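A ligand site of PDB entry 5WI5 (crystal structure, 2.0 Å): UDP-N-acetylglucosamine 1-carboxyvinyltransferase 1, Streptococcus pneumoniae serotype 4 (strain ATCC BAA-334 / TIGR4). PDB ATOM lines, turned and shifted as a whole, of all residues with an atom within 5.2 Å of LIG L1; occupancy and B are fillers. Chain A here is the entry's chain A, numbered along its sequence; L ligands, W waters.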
ATOM      1  N   LYS A  26     -41.781  -3.123 -11.872  1.00  0.00           N
ATOM      2  CA  LYS A  26     -41.675  -1.677 -11.667  1.00  0.00           C
ATOM      3  C   LYS A  26     -40.720  -1.090 -12.692  1.00  0.00           C
ATOM      4  O   LYS A  26     -41.013  -0.056 -13.283  1.00  0.00           O
ATOM      5  CB  LYS A  26     -41.081  -1.409 -10.297  1.00  0.00           C
ATOM      6  CG  LYS A  26     -40.592   0.022 -10.019  1.00  0.00           C
ATOM      7  CD  LYS A  26     -39.478  -0.121  -8.981  1.00  0.00           C
ATOM      8  CE  LYS A  26     -38.688   1.102  -8.678  1.00  0.00           C
ATOM      9  NZ  LYS A  26     -37.751   1.469  -9.724  1.00  0.00           N
ATOM     10  N   ASN A  27     -39.586  -1.764 -12.906  1.00  0.00           N
ATOM     11  CA  ASN A  27     -38.557  -1.221 -13.827  1.00  0.00           C
ATOM     12  C   ASN A  27     -38.840  -1.462 -15.302  1.00  0.00           C
ATOM     13  O   ASN A  27     -38.074  -1.024 -16.163  1.00  0.00           O
ATOM     14  CB  ASN A  27     -37.144  -1.684 -13.403  1.00  0.00           C
ATOM     15  CG  ASN A  27     -36.654  -0.960 -12.168  1.00  0.00           C
ATOM     16  OD1 ASN A  27     -37.238   0.029 -11.738  1.00  0.00           O
ATOM     17  ND2 ASN A  27     -35.565  -1.436 -11.592  1.00  0.00           N
ATOM     18  N   LEU A  30     -41.964   1.689 -15.734  1.00  0.00           N
ATOM     19  CA  LEU A  30     -41.493   3.056 -15.843  1.00  0.00           C
ATOM     20  C   LEU A  30     -41.112   3.449 -17.278  1.00  0.00           C
ATOM     21  O   LEU A  30     -41.627   4.434 -17.791  1.00  0.00           O
ATOM     22  CB  LEU A  30     -40.386   3.395 -14.832  1.00  0.00           C
ATOM     23  CG  LEU A  30     -40.686   3.247 -13.347  1.00  0.00           C
ATOM     24  CD1 LEU A  30     -39.555   3.872 -12.538  1.00  0.00           C
ATOM     25  CD2 LEU A  30     -42.018   3.813 -12.967  1.00  0.00           C
ATOM     26  N   ASP A  54     -43.345   4.848  -7.402  1.00  0.00           N
ATOM     27  CA  ASP A  54     -42.616   5.207  -8.630  1.00  0.00           C
ATOM     28  C   ASP A  54     -43.532   5.257  -9.840  1.00  0.00           C
ATOM     29  O   ASP A  54     -43.284   6.050 -10.745  1.00  0.00           O
ATOM     30  CB  ASP A  54     -41.419   4.248  -8.902  1.00  0.00           C
ATOM     31  CG  ASP A  54     -40.158   4.586  -8.045  1.00  0.00           C
ATOM     32  OD1 ASP A  54     -40.225   5.414  -7.129  1.00  0.00           O
ATOM     33  OD2 ASP A  54     -39.095   4.000  -8.323  1.00  0.00           O
ATOM     34  N   ALA A 100     -35.202   8.331 -12.340  1.00  0.00           N
ATOM     35  CA  ALA A 100     -35.642   7.495 -13.484  1.00  0.00           C
ATOM     36  C   ALA A 100     -36.587   8.253 -14.393  1.00  0.00           C
ATOM     37  O   ALA A 100     -36.843   7.829 -15.522  1.00  0.00           O
ATOM     38  CB  ALA A 100     -36.301   6.218 -12.997  1.00  0.00           C
ATOM     39  N   ILE A 125     -26.955   5.759  -3.483  1.00  0.00           N
ATOM     40  CA  ILE A 125     -26.373   4.436  -3.829  1.00  0.00           C
ATOM     41  C   ILE A 125     -25.155   4.507  -4.754  1.00  0.00           C
ATOM     42  O   ILE A 125     -24.485   3.489  -4.994  1.00  0.00           O
ATOM     43  CB  ILE A 125     -27.398   3.405  -4.356  1.00  0.00           C
ATOM     44  CG1 ILE A 125     -27.950   3.753  -5.736  1.00  0.00           C
ATOM     45  CG2 ILE A 125     -28.553   3.224  -3.341  1.00  0.00           C
ATOM     46  CD1 ILE A 125     -28.676   2.585  -6.366  1.00  0.00           C
ATOM     47  N   SER A 127     -22.686   7.353  -7.699  1.00  0.00           N
ATOM     48  CA  SER A 127     -22.506   8.542  -8.520  1.00  0.00           C
ATOM     49  C   SER A 127     -23.562   8.784  -9.592  1.00  0.00           C
ATOM     50  O   SER A 127     -23.912   9.893  -9.827  1.00  0.00           O
ATOM     51  CB  SER A 127     -21.139   8.505  -9.199  1.00  0.00           C
ATOM     52  OG  SER A 127     -21.007   9.650  -9.994  1.00  0.00           O
ATOM     53  N   ARG A 128     -23.953   7.788 -10.326  1.00  0.00           N
ATOM     54  CA  ARG A 128     -25.100   7.897 -11.316  1.00  0.00           C
ATOM     55  C   ARG A 128     -25.136   9.026 -12.353  1.00  0.00           C
ATOM     56  O   ARG A 128     -26.157   9.693 -12.548  1.00  0.00           O
ATOM     57  CB  ARG A 128     -26.512   7.746 -10.656  1.00  0.00           C
ATOM     58  CG  ARG A 128     -26.524   6.563  -9.699  1.00  0.00           C
ATOM     59  CD  ARG A 128     -27.868   6.269  -9.155  1.00  0.00           C
ATOM     60  NE  ARG A 128     -28.710   5.582 -10.109  1.00  0.00           N
ATOM     61  CZ  ARG A 128     -29.896   5.062  -9.817  1.00  0.00           C
ATOM     62  NH1 ARG A 128     -30.413   5.224  -8.602  1.00  0.00           N
ATOM     63  NH2 ARG A 128     -30.582   4.396 -10.754  1.00  0.00           N
ATOM     64  N   PRO A 129     -24.019   9.189 -13.076  1.00  0.00           N
ATOM     65  CA  PRO A 129     -23.976  10.191 -14.143  1.00  0.00           C
ATOM     66  C   PRO A 129     -24.840   9.753 -15.324  1.00  0.00           C
ATOM     67  O   PRO A 129     -25.226   8.580 -15.417  1.00  0.00           O
ATOM     68  CB  PRO A 129     -22.505  10.232 -14.517  1.00  0.00           C
ATOM     69  CG  PRO A 129     -21.998   8.861 -14.200  1.00  0.00           C
ATOM     70  CD  PRO A 129     -22.747   8.454 -12.971  1.00  0.00           C
ATOM     71  N   ILE A 130     -25.158  10.688 -16.196  1.00  0.00           N
ATOM     72  CA  ILE A 130     -26.000  10.405 -17.362  1.00  0.00           C
ATOM     73  C   ILE A 130     -25.287  10.738 -18.667  1.00  0.00           C
ATOM     74  O   ILE A 130     -25.928  10.854 -19.730  1.00  0.00           O
ATOM     75  CB  ILE A 130     -27.349  11.131 -17.284  1.00  0.00           C
ATOM     76  CG1 ILE A 130     -27.157  12.652 -17.257  1.00  0.00           C
ATOM     77  CG2 ILE A 130     -28.099  10.697 -16.040  1.00  0.00           C
ATOM     78  CD1 ILE A 130     -28.438  13.441 -17.431  1.00  0.00           C
ATOM     79  N   ASP A 131     -23.950  10.833 -18.605  1.00  0.00           N
ATOM     80  CA  ASP A 131     -23.136  11.136 -19.796  1.00  0.00           C
ATOM     81  C   ASP A 131     -23.482  10.268 -21.012  1.00  0.00           C
ATOM     82  O   ASP A 131     -23.477  10.760 -22.137  1.00  0.00           O
ATOM     83  CB  ASP A 131     -21.615  11.012 -19.489  1.00  0.00           C
ATOM     84  CG  ASP A 131     -21.178   9.562 -19.059  1.00  0.00           C
ATOM     85  OD1 ASP A 131     -21.625   9.050 -17.997  1.00  0.00           O
ATOM     86  OD2 ASP A 131     -20.337   8.938 -19.754  1.00  0.00           O
ATOM     87  N   LEU A 132     -23.779   8.984 -20.801  1.00  0.00           N
ATOM     88  CA  LEU A 132     -24.086   8.071 -21.909  1.00  0.00           C
ATOM     89  C   LEU A 132     -25.381   8.441 -22.609  1.00  0.00           C
ATOM     90  O   LEU A 132     -25.477   8.276 -23.830  1.00  0.00           O
ATOM     91  CB  LEU A 132     -24.102   6.612 -21.475  1.00  0.00           C
ATOM     92  CG  LEU A 132     -22.824   6.077 -20.834  1.00  0.00           C
ATOM     93  CD1 LEU A 132     -22.999   4.603 -20.447  1.00  0.00           C
ATOM     94  CD2 LEU A 132     -21.633   6.208 -21.782  1.00  0.00           C
ATOM     95  N   HIS A 133     -26.362   8.947 -21.863  1.00  0.00           N
ATOM     96  CA  HIS A 133     -27.602   9.374 -22.463  1.00  0.00           C
ATOM     97  C   HIS A 133     -27.344  10.551 -23.411  1.00  0.00           C
ATOM     98  O   HIS A 133     -27.722  10.530 -24.571  1.00  0.00           O
ATOM     99  CB  HIS A 133     -28.598   9.895 -21.421  1.00  0.00           C
ATOM    100  CG  HIS A 133     -29.066   8.900 -20.423  1.00  0.00           C
ATOM    101  ND1 HIS A 133     -30.372   8.492 -20.378  1.00  0.00           N
ATOM    102  CD2 HIS A 133     -28.437   8.299 -19.384  1.00  0.00           C
ATOM    103  CE1 HIS A 133     -30.542   7.641 -19.372  1.00  0.00           C
ATOM    104  NE2 HIS A 133     -29.379   7.514 -18.752  1.00  0.00           N
ATOM    105  N   PHE A 167     -20.544   1.622 -21.382  1.00  0.00           N
ATOM    106  CA  PHE A 167     -21.122   0.696 -20.405  1.00  0.00           C
ATOM    107  C   PHE A 167     -22.552   0.450 -20.824  1.00  0.00           C
ATOM    108  O   PHE A 167     -23.206   1.380 -21.302  1.00  0.00           O
ATOM    109  CB  PHE A 167     -21.063   1.333 -19.002  1.00  0.00           C
ATOM    110  CG  PHE A 167     -21.596   0.445 -17.917  1.00  0.00           C
ATOM    111  CD1 PHE A 167     -20.765  -0.477 -17.273  1.00  0.00           C
ATOM    112  CD2 PHE A 167     -22.923   0.533 -17.521  1.00  0.00           C
ATOM    113  CE1 PHE A 167     -21.271  -1.318 -16.295  1.00  0.00           C
ATOM    114  CE2 PHE A 167     -23.429  -0.310 -16.532  1.00  0.00           C
ATOM    115  CZ  PHE A 167     -22.599  -1.238 -15.921  1.00  0.00           C
ATOM    116  N   PRO A 168     -23.060  -0.765 -20.642  1.00  0.00           N
ATOM    117  CA  PRO A 168     -24.454  -1.059 -21.077  1.00  0.00           C
ATOM    118  C   PRO A 168     -25.539  -0.505 -20.162  1.00  0.00           C
ATOM    119  O   PRO A 168     -26.283  -1.260 -19.516  1.00  0.00           O
ATOM    120  CB  PRO A 168     -24.460  -2.588 -21.129  1.00  0.00           C
ATOM    121  CG  PRO A 168     -23.482  -3.005 -20.089  1.00  0.00           C
ATOM    122  CD  PRO A 168     -22.369  -1.999 -20.222  1.00  0.00           C
ATOM    123  N   SER A 169     -25.629   0.807 -20.109  1.00  0.00           N
ATOM    124  CA  SER A 169     -26.620   1.490 -19.257  1.00  0.00           C
ATOM    125  C   SER A 169     -28.026   1.131 -19.623  1.00  0.00           C
ATOM    126  O   SER A 169     -28.421   1.235 -20.793  1.00  0.00           O
ATOM    127  CB  SER A 169     -26.456   3.001 -19.344  1.00  0.00           C
ATOM    128  OG  SER A 169     -27.553   3.695 -18.797  1.00  0.00           O
ATOM    129  N   VAL A 170     -28.791   0.683 -18.609  1.00  0.00           N
ATOM    130  CA  VAL A 170     -30.212   0.370 -18.797  1.00  0.00           C
ATOM    131  C   VAL A 170     -30.955   1.623 -19.268  1.00  0.00           C
ATOM    132  O   VAL A 170     -31.568   1.622 -20.342  1.00  0.00           O
ATOM    133  CB  VAL A 170     -30.814  -0.160 -17.460  1.00  0.00           C
ATOM    134  CG1 VAL A 170     -32.331  -0.203 -17.497  1.00  0.00           C
ATOM    135  CG2 VAL A 170     -30.219  -1.533 -17.135  1.00  0.00           C
ATOM    136  N   GLY A 171     -30.856   2.700 -18.488  1.00  0.00           N
ATOM    137  CA  GLY A 171     -31.539   3.944 -18.771  1.00  0.00           C
ATOM    138  C   GLY A 171     -31.151   4.575 -20.097  1.00  0.00           C
ATOM    139  O   GLY A 171     -32.015   5.007 -20.868  1.00  0.00           O
ATOM    140  N   ALA A 172     -29.856   4.639 -20.360  1.00  0.00           N
ATOM    141  CA  ALA A 172     -29.385   5.211 -21.607  1.00  0.00           C
ATOM    142  C   ALA A 172     -29.874   4.390 -22.783  1.00  0.00           C
ATOM    143  O   ALA A 172     -30.348   4.958 -23.767  1.00  0.00           O
ATOM    144  CB  ALA A 172     -27.882   5.349 -21.628  1.00  0.00           C
ATOM    145  N   GLN A 174     -32.565   2.618 -22.959  1.00  0.00           N
ATOM    146  CA  GLN A 174     -33.999   2.901 -23.082  1.00  0.00           C
ATOM    147  C   GLN A 174     -34.263   4.251 -23.756  1.00  0.00           C
ATOM    148  O   GLN A 174     -35.063   4.310 -24.677  1.00  0.00           O
ATOM    149  CB  GLN A 174     -34.673   2.814 -21.701  1.00  0.00           C
ATOM    150  CG  GLN A 174     -34.677   1.380 -21.159  1.00  0.00           C
ATOM    151  CD  GLN A 174     -35.034   1.290 -19.705  1.00  0.00           C
ATOM    152  OE1 GLN A 174     -35.056   2.290 -18.991  1.00  0.00           O
ATOM    153  NE2 GLN A 174     -35.302   0.070 -19.243  1.00  0.00           N
ATOM    154  N   GLU A 195     -30.973  -6.245 -20.288  1.00  0.00           N
ATOM    155  CA  GLU A 195     -31.965  -6.594 -19.262  1.00  0.00           C
ATOM    156  C   GLU A 195     -33.326  -7.005 -19.823  1.00  0.00           C
ATOM    157  O   GLU A 195     -33.719  -6.512 -20.867  1.00  0.00           O
ATOM    158  CB  GLU A 195     -32.145  -5.437 -18.262  1.00  0.00           C
ATOM    159  CG  GLU A 195     -31.191  -5.401 -17.077  1.00  0.00           C
ATOM    160  CD  GLU A 195     -29.739  -5.129 -17.412  1.00  0.00           C
ATOM    161  OE1 GLU A 195     -29.406  -4.651 -18.529  1.00  0.00           O
ATOM    162  OE2 GLU A 195     -28.890  -5.373 -16.490  1.00  0.00           O
ATOM    163  N   THR A 311     -27.613  -6.417  -9.781  1.00  0.00           N
ATOM    164  CA  THR A 311     -27.355  -5.592  -8.595  1.00  0.00           C
ATOM    165  C   THR A 311     -28.630  -5.444  -7.775  1.00  0.00           C
ATOM    166  O   THR A 311     -28.554  -5.289  -6.554  1.00  0.00           O
ATOM    167  CB  THR A 311     -26.779  -4.210  -8.973  1.00  0.00           C
ATOM    168  OG1 THR A 311     -26.636  -3.399  -7.807  1.00  0.00           O
ATOM    169  CG2 THR A 311     -27.678  -3.469  -9.985  1.00  0.00           C
ATOM    170  N   ASP A 312     -29.782  -5.517  -8.446  1.00  0.00           N
ATOM    171  CA  ASP A 312     -31.074  -5.413  -7.749  1.00  0.00           C
ATOM    172  C   ASP A 312     -31.432  -6.621  -6.859  1.00  0.00           C
ATOM    173  O   ASP A 312     -32.386  -6.559  -6.101  1.00  0.00           O
ATOM    174  CB  ASP A 312     -32.212  -5.123  -8.748  1.00  0.00           C
ATOM    175  CG  ASP A 312     -32.268  -3.643  -9.136  1.00  0.00           C
ATOM    176  OD1 ASP A 312     -31.513  -2.782  -8.585  1.00  0.00           O
ATOM    177  OD2 ASP A 312     -33.110  -3.338 -10.003  1.00  0.00           O
ATOM    178  N   VAL A 334     -21.732  -2.510 -10.004  1.00  0.00           N
ATOM    179  CA  VAL A 334     -22.615  -1.623 -10.744  1.00  0.00           C
ATOM    180  C   VAL A 334     -22.765  -0.246 -10.108  1.00  0.00           C
ATOM    181  O   VAL A 334     -22.725   0.739 -10.805  1.00  0.00           O
ATOM    182  CB  VAL A 334     -23.987  -2.299 -10.984  1.00  0.00           C
ATOM    183  CG1 VAL A 334     -24.914  -1.396 -11.787  1.00  0.00           C
ATOM    184  CG2 VAL A 334     -23.758  -3.625 -11.680  1.00  0.00           C
ATOM    185  N   PHE A 335     -22.926  -0.208  -8.792  1.00  0.00           N
ATOM    186  CA  PHE A 335     -23.056   1.028  -8.058  1.00  0.00           C
ATOM    187  C   PHE A 335     -21.950   1.050  -7.000  1.00  0.00           C
ATOM    188  O   PHE A 335     -21.570   0.004  -6.505  1.00  0.00           O
ATOM    189  CB  PHE A 335     -24.432   1.110  -7.387  1.00  0.00           C
ATOM    190  CG  PHE A 335     -25.576   1.252  -8.359  1.00  0.00           C
ATOM    191  CD1 PHE A 335     -25.792   2.463  -9.011  1.00  0.00           C
ATOM    192  CD2 PHE A 335     -26.425   0.202  -8.623  1.00  0.00           C
ATOM    193  CE1 PHE A 335     -26.839   2.624  -9.907  1.00  0.00           C
ATOM    194  CE2 PHE A 335     -27.461   0.341  -9.516  1.00  0.00           C
ATOM    195  CZ  PHE A 335     -27.678   1.564 -10.154  1.00  0.00           C
ATOM    196  N   GLU A 336     -21.489   2.240  -6.643  1.00  0.00           N
ATOM    197  CA  GLU A 336     -20.376   2.373  -5.693  1.00  0.00           C
ATOM    198  C   GLU A 336     -20.744   2.350  -4.220  1.00  0.00           C
ATOM    199  O   GLU A 336     -19.863   2.084  -3.391  1.00  0.00           O
ATOM    200  CB  GLU A 336     -19.596   3.687  -5.937  1.00  0.00           C
ATOM    201  CG  GLU A 336     -19.013   3.875  -7.313  1.00  0.00           C
ATOM    202  CD  GLU A 336     -19.930   4.555  -8.327  1.00  0.00           C
ATOM    203  OE1 GLU A 336     -21.172   4.602  -8.138  1.00  0.00           O
ATOM    204  OE2 GLU A 336     -19.364   5.034  -9.329  1.00  0.00           O
ATOM    205  N   ARG A 338     -23.667   0.749  -2.480  1.00  0.00           N
ATOM    206  CA  ARG A 338     -24.891  -0.025  -2.286  1.00  0.00           C
ATOM    207  C   ARG A 338     -24.756  -1.141  -1.238  1.00  0.00           C
ATOM    208  O   ARG A 338     -25.313  -2.233  -1.383  1.00  0.00           O
ATOM    209  CB  ARG A 338     -25.377  -0.587  -3.627  1.00  0.00           C
ATOM    210  CG  ARG A 338     -26.859  -0.846  -3.638  1.00  0.00           C
ATOM    211  CD  ARG A 338     -27.359  -1.364  -4.957  1.00  0.00           C
ATOM    212  NE  ARG A 338     -28.806  -1.425  -4.965  1.00  0.00           N
ATOM    213  CZ  ARG A 338     -29.549  -1.760  -6.011  1.00  0.00           C
ATOM    214  NH1 ARG A 338     -28.983  -2.153  -7.164  1.00  0.00           N
ATOM    215  NH2 ARG A 338     -30.879  -1.737  -5.900  1.00  0.00           N
ATOM    216  N   LEU A 377     -34.671   1.166  -1.744  1.00  0.00           N
ATOM    217  CA  LEU A 377     -35.671   0.134  -2.057  1.00  0.00           C
ATOM    218  C   LEU A 377     -35.271  -1.322  -1.737  1.00  0.00           C
ATOM    219  O   LEU A 377     -35.933  -1.986  -0.935  1.00  0.00           O
ATOM    220  CB  LEU A 377     -36.047   0.273  -3.541  1.00  0.00           C
ATOM    221  CG  LEU A 377     -36.923  -0.817  -4.143  1.00  0.00           C
ATOM    222  CD1 LEU A 377     -38.195  -1.042  -3.342  1.00  0.00           C
ATOM    223  CD2 LEU A 377     -37.257  -0.466  -5.592  1.00  0.00           C
ATOM    224  N   ARG A 378     -34.215  -1.826  -2.357  1.00  0.00           N
ATOM    225  CA  ARG A 378     -33.823  -3.211  -2.144  1.00  0.00           C
ATOM    226  C   ARG A 378     -33.258  -3.471  -0.754  1.00  0.00           C
ATOM    227  O   ARG A 378     -33.397  -4.562  -0.194  1.00  0.00           O
ATOM    228  CB  ARG A 378     -32.872  -3.675  -3.259  1.00  0.00           C
ATOM    229  CG  ARG A 378     -33.408  -3.458  -4.663  1.00  0.00           C
ATOM    230  CD  ARG A 378     -34.827  -4.038  -4.905  1.00  0.00           C
ATOM    231  NE  ARG A 378     -35.343  -3.663  -6.221  1.00  0.00           N
ATOM    232  CZ  ARG A 378     -36.564  -3.929  -6.682  1.00  0.00           C
ATOM    233  NH1 ARG A 378     -37.449  -4.595  -5.955  1.00  0.00           N
ATOM    234  NH2 ARG A 378     -36.921  -3.548  -7.892  1.00  0.00           N
ATOM    235  N   ARG A 404     -41.689   2.052  -3.036  1.00  0.00           N
ATOM    236  CA  ARG A 404     -41.339   2.407  -4.404  1.00  0.00           C
ATOM    237  C   ARG A 404     -41.335   1.190  -5.314  1.00  0.00           C
ATOM    238  O   ARG A 404     -41.565   1.327  -6.507  1.00  0.00           O
ATOM    239  CB  ARG A 404     -39.964   3.089  -4.463  1.00  0.00           C
ATOM    240  CG  ARG A 404     -39.941   4.448  -3.791  1.00  0.00           C
ATOM    241  CD  ARG A 404     -38.585   5.082  -3.849  1.00  0.00           C
ATOM    242  NE  ARG A 404     -38.178   5.359  -5.222  1.00  0.00           N
ATOM    243  CZ  ARG A 404     -37.047   5.961  -5.550  1.00  0.00           C
ATOM    244  NH1 ARG A 404     -36.182   6.335  -4.603  1.00  0.00           N
ATOM    245  NH2 ARG A 404     -36.769   6.167  -6.821  1.00  0.00           N
HETATM  246  N1  LIG L   1     -23.753   4.890 -15.863  1.00  0.00           N
HETATM  247  C1  LIG L   1     -22.821   5.841 -16.318  1.00  0.00           C
HETATM  248  N2  LIG L   1     -23.199   6.737 -17.223  1.00  0.00           N
HETATM  249  C2  LIG L   1     -24.451   6.772 -17.720  1.00  0.00           C
HETATM  250  C3  LIG L   1     -25.404   5.850 -17.276  1.00  0.00           C
HETATM  251  C4  LIG L   1     -25.023   4.921 -16.327  1.00  0.00           C
HETATM  252  O1  LIG L   1     -21.662   5.847 -15.893  1.00  0.00           O
HETATM  253  O2  LIG L   1     -24.741   7.646 -18.569  1.00  0.00           O
HETATM  254  C5  LIG L   1     -23.376   3.939 -14.836  1.00  0.00           C
HETATM  255  C6  LIG L   1     -24.107   4.410 -13.581  1.00  0.00           C
HETATM  256  O3  LIG L   1     -23.369   5.300 -12.730  1.00  0.00           O
HETATM  257  C7  LIG L   1     -24.402   3.135 -12.870  1.00  0.00           C
HETATM  258  C8  LIG L   1     -24.311   2.049 -13.915  1.00  0.00           C
HETATM  259  O4  LIG L   1     -23.865   2.638 -15.155  1.00  0.00           O
HETATM  260  O5  LIG L   1     -23.457   2.966 -11.838  1.00  0.00           O
HETATM  261  C9  LIG L   1     -25.655   1.396 -14.112  1.00  0.00           C
HETATM  262  O6  LIG L   1     -26.633   2.388 -14.358  1.00  0.00           O
HETATM  263  P1  LIG L   1     -27.803   2.108 -15.378  1.00  0.00           P
HETATM  264  O7  LIG L   1     -27.942   3.323 -16.245  1.00  0.00           O
HETATM  265  O8  LIG L   1     -27.633   0.713 -15.989  1.00  0.00           O
HETATM  266  O9  LIG L   1     -29.027   1.961 -14.336  1.00  0.00           O
HETATM  267  P2  LIG L   1     -30.286   2.952 -14.308  1.00  0.00           P
HETATM  268  O10 LIG L   1     -31.012   2.936 -15.651  1.00  0.00           O
HETATM  269  O11 LIG L   1     -29.871   4.216 -13.646  1.00  0.00           O
HETATM  270  C10 LIG L   1     -31.857   0.915 -13.653  1.00  0.00           C
HETATM  271  C11 LIG L   1     -32.865   0.595 -12.577  1.00  0.00           C
HETATM  272  C12 LIG L   1     -32.135   0.377 -11.271  1.00  0.00           C
HETATM  273  C13 LIG L   1     -31.196  -0.819 -11.454  1.00  0.00           C
HETATM  274  C14 LIG L   1     -30.203  -0.461 -12.539  1.00  0.00           C
HETATM  275  C15 LIG L   1     -29.150  -1.555 -12.867  1.00  0.00           C
HETATM  276  C16 LIG L   1     -34.889   1.700 -13.348  1.00  0.00           C
HETATM  277  C17 LIG L   1     -35.935   2.756 -13.123  1.00  0.00           C
HETATM  278  N3  LIG L   1     -33.886   1.614 -12.479  1.00  0.00           N
HETATM  279  O12 LIG L   1     -31.199   2.137 -13.292  1.00  0.00           O
HETATM  280  O13 LIG L   1     -33.155   0.109 -10.315  1.00  0.00           O
HETATM  281  O14 LIG L   1     -30.493  -1.039 -10.238  1.00  0.00           O
HETATM  282  O15 LIG L   1     -30.892  -0.152 -13.746  1.00  0.00           O
HETATM  283  O16 LIG L   1     -29.720  -2.790 -13.149  1.00  0.00           O
HETATM  284  O17 LIG L   1     -34.987   0.945 -14.277  1.00  0.00           O
HETATM  285  C18 LIG L   1     -34.630   1.387  -8.800  1.00  0.00           C
HETATM  286  O18 LIG L   1     -35.501   0.508  -8.853  1.00  0.00           O
HETATM  287  O19 LIG L   1     -34.879   2.566  -8.428  1.00  0.00           O
HETATM  288  C19 LIG L   1     -33.294   0.906  -9.107  1.00  0.00           C
HETATM  289  C20 LIG L   1     -32.335   0.993  -8.191  1.00  0.00           C
HETATM  290  C1  LG2 L   2     -31.578   8.638  -4.165  1.00  0.00           C
HETATM  291  O1  LG2 L   2     -30.912   8.420  -3.121  1.00  0.00           O
HETATM  292  O2  LG2 L   2     -32.327   9.655  -4.278  1.00  0.00           O
HETATM  293  C2  LG2 L   2     -31.374   7.646  -5.295  1.00  0.00           C
HETATM  294  C3  LG2 L   2     -31.928   6.287  -4.852  1.00  0.00           C
HETATM  295  O3  LG2 L   2     -31.947   8.041  -6.557  1.00  0.00           O
HETATM  296  P1  LG2 L   2     -33.542   8.191  -6.837  1.00  0.00           P
HETATM  297  O4  LG2 L   2     -34.045   7.006  -7.603  1.00  0.00           O
HETATM  298  O5  LG2 L   2     -33.731   9.467  -7.632  1.00  0.00           O
HETATM  299  O6  LG2 L   2     -34.339   8.257  -5.549  1.00  0.00           O
HETATM  300  O   HOH W   1     -35.678   2.846 -16.453  1.00  0.00           O
HETATM  301  O   HOH W   2     -26.634  -1.837 -15.889  1.00  0.00           O
HETATM  302  O   HOH W   3     -32.391  -3.566 -14.163  1.00  0.00           O
HETATM  303  O   HOH W   4     -34.692  -1.835  -8.398  1.00  0.00           O
HETATM  304  O   HOH W   5     -30.230  -5.265 -11.543  1.00  0.00           O
HETATM  305  O   HOH W   6     -27.852  -3.847 -14.640  1.00  0.00           O
HETATM  306  O   HOH W   7     -23.042   4.703  -9.972  1.00  0.00           O
HETATM  307  O   HOH W   8     -33.276   4.363 -15.607  1.00  0.00           O
HETATM  308  O   HOH W   9     -27.650   5.099 -12.591  1.00  0.00           O
HETATM  309  O   HOH W  10     -32.575   5.634 -13.259  1.00  0.00           O
HETATM  310  O   HOH W  11     -36.890   4.479  -9.666  1.00  0.00           O
HETATM  311  O   HOH W  12     -35.389  -0.757 -16.520  1.00  0.00           O
HETATM  312  O   HOH W  13     -21.006   5.445 -11.821  1.00  0.00           O
HETATM  313  O   HOH W  14     -28.966   5.749 -16.311  1.00  0.00           O
HETATM  314  O   HOH W  15     -33.042   4.471  -7.696  1.00  0.00           O
HETATM  315  O   HOH W  16     -36.339   2.848  -6.080  1.00  0.00           O
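Leu 30 touches LIG L1 (CD1 to C17, 3.8 Å). CB of Ala 100 touches C17 of LIG L1 (3.5 Å). Ile 130 touches LIG L1 (C to O2, 3.1 Å). His 133 touches LIG L1 (CD2 to O2, 3.8 Å). CE2 of Phe 167 touches O4 of LIG L1, at 3.3 Å. Thr 311 touches LIG L1 (CG2 to O14, 3.7 Å). Phe 335 touches LIG L1. NH1 of Arg 338 touches O14 of LIG L1 (3.6 Å). Leu 377 touches LIG L1. The nearest printed residue that does not touch LIG L1 is Pro 168 (4.3 Å).
The side-chain amide oxygen (OD1) of Asn 27 lies within hydrogen-bond range of the side-chain amino group (NZ) of Lys 26, 2.5 Å away. The side-chain amino group of Lys 26 lies within salt-bridge range of the side-chain carboxylate of Asp 54, at 3.2 Å. The backbone NH (N) of Gly 171 lies close to the side-chain hydroxyl (OG) of Ser 169, 3.5 Å away. OG of Ser 169 is in hydrogen-bond range of N of Ala 172 (2.9 Å). The side-chain carboxylate (OD2) of Asp 312 sits at hydrogen-bond distance from the side-chain amide nitrogen (ND2) of Asn 27. NH2 of Arg 338 is in salt-bridge range of OD1 of Asp 312. The guanidinium group (NH1) of Arg 338 sits at hydrogen-bond distance from the side-chain hydroxyl (OG1) of Thr 311, 2.7 Å away. The backbone NH (N) of Ala 172 lies close to a ring nitrogen (NE2) of His 133 (3.3 Å).
Water W4 lies within hydrogen-bond range of an oxygen (O18) of LIG L1 (2.5 Å), the side-chain carboxylate of Asp 312 (2.7 Å), the guanidinium group of Arg 378 (2.9 Å) and the side-chain amide nitrogen of Asn 27 (3.3 Å). Water W13 bridges an oxygen (O3) of LIG L1 (2.5 Å) and the side-chain carboxylate (OE2) of Glu 336 (3.0 Å). Water W14 bridges an oxygen (O7) of LIG L1 (2.6 Å) and a ring nitrogen (NE2) of His 133 (3.0 Å). Water W5 lies within hydrogen-bond range of an oxygen (O16) of LIG L1 (3.0 Å), the backbone NH (N) of Asp 312 (3.1 Å) and the backbone NH (N) of Thr 311 (3.4 Å). Water W11 lies within hydrogen-bond range of the side-chain carboxylate of Asp 54, an oxygen (O19) of LIG L1, the side-chain amino group of Lys 26 and the guanidinium group of Arg 404. Water W10 lies within hydrogen-bond range of an oxygen (O11) of LIG L1 and the guanidinium group (NH2) of Arg 128.
O of Val 334 sits at hydrogen-bond distance from O5 of LIG L1, 2.6 Å away. O18 of LIG L1 lies within salt-bridge range of NZ of Lys 26. OG of Ser 169 lies within hydrogen-bond range of O7 of LIG L1 (2.6 Å). An oxygen (O14) of LIG L1 sits at hydrogen-bond distance from the side-chain carboxylate (OD1) of Asp 312 (2.6 Å). N of Leu 132 lies within hydrogen-bond range of O2 of LIG L1, 2.8 Å away. N of Gly 171 is in hydrogen-bond range of O10 of LIG L1 (2.9 Å). An oxygen (O8) of LIG L1 lies within hydrogen-bond range of the backbone NH of Val 170 (2.9 Å). An oxygen (O2) of LIG L1 is in hydrogen-bond range of the backbone NH of Asp 131 (3.3 Å). The side-chain carboxylate of Asp 131 sits at hydrogen-bond distance from a nitrogen (N2) of LIG L1. An oxygen (O11) of LIG L1 lies within salt-bridge range of the guanidinium group (NH2) of Arg 128 (3.0 Å). N2 of LIG L1 sits close to O of Pro 129 (3.3 Å). ND2 of Asn 27 is in hydrogen-bond range of O13 of LIG L1. The guanidinium group (NH2) of Arg 404 lies within salt-bridge range of an oxygen (O4) of LG2 L2, at 3.0 Å.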
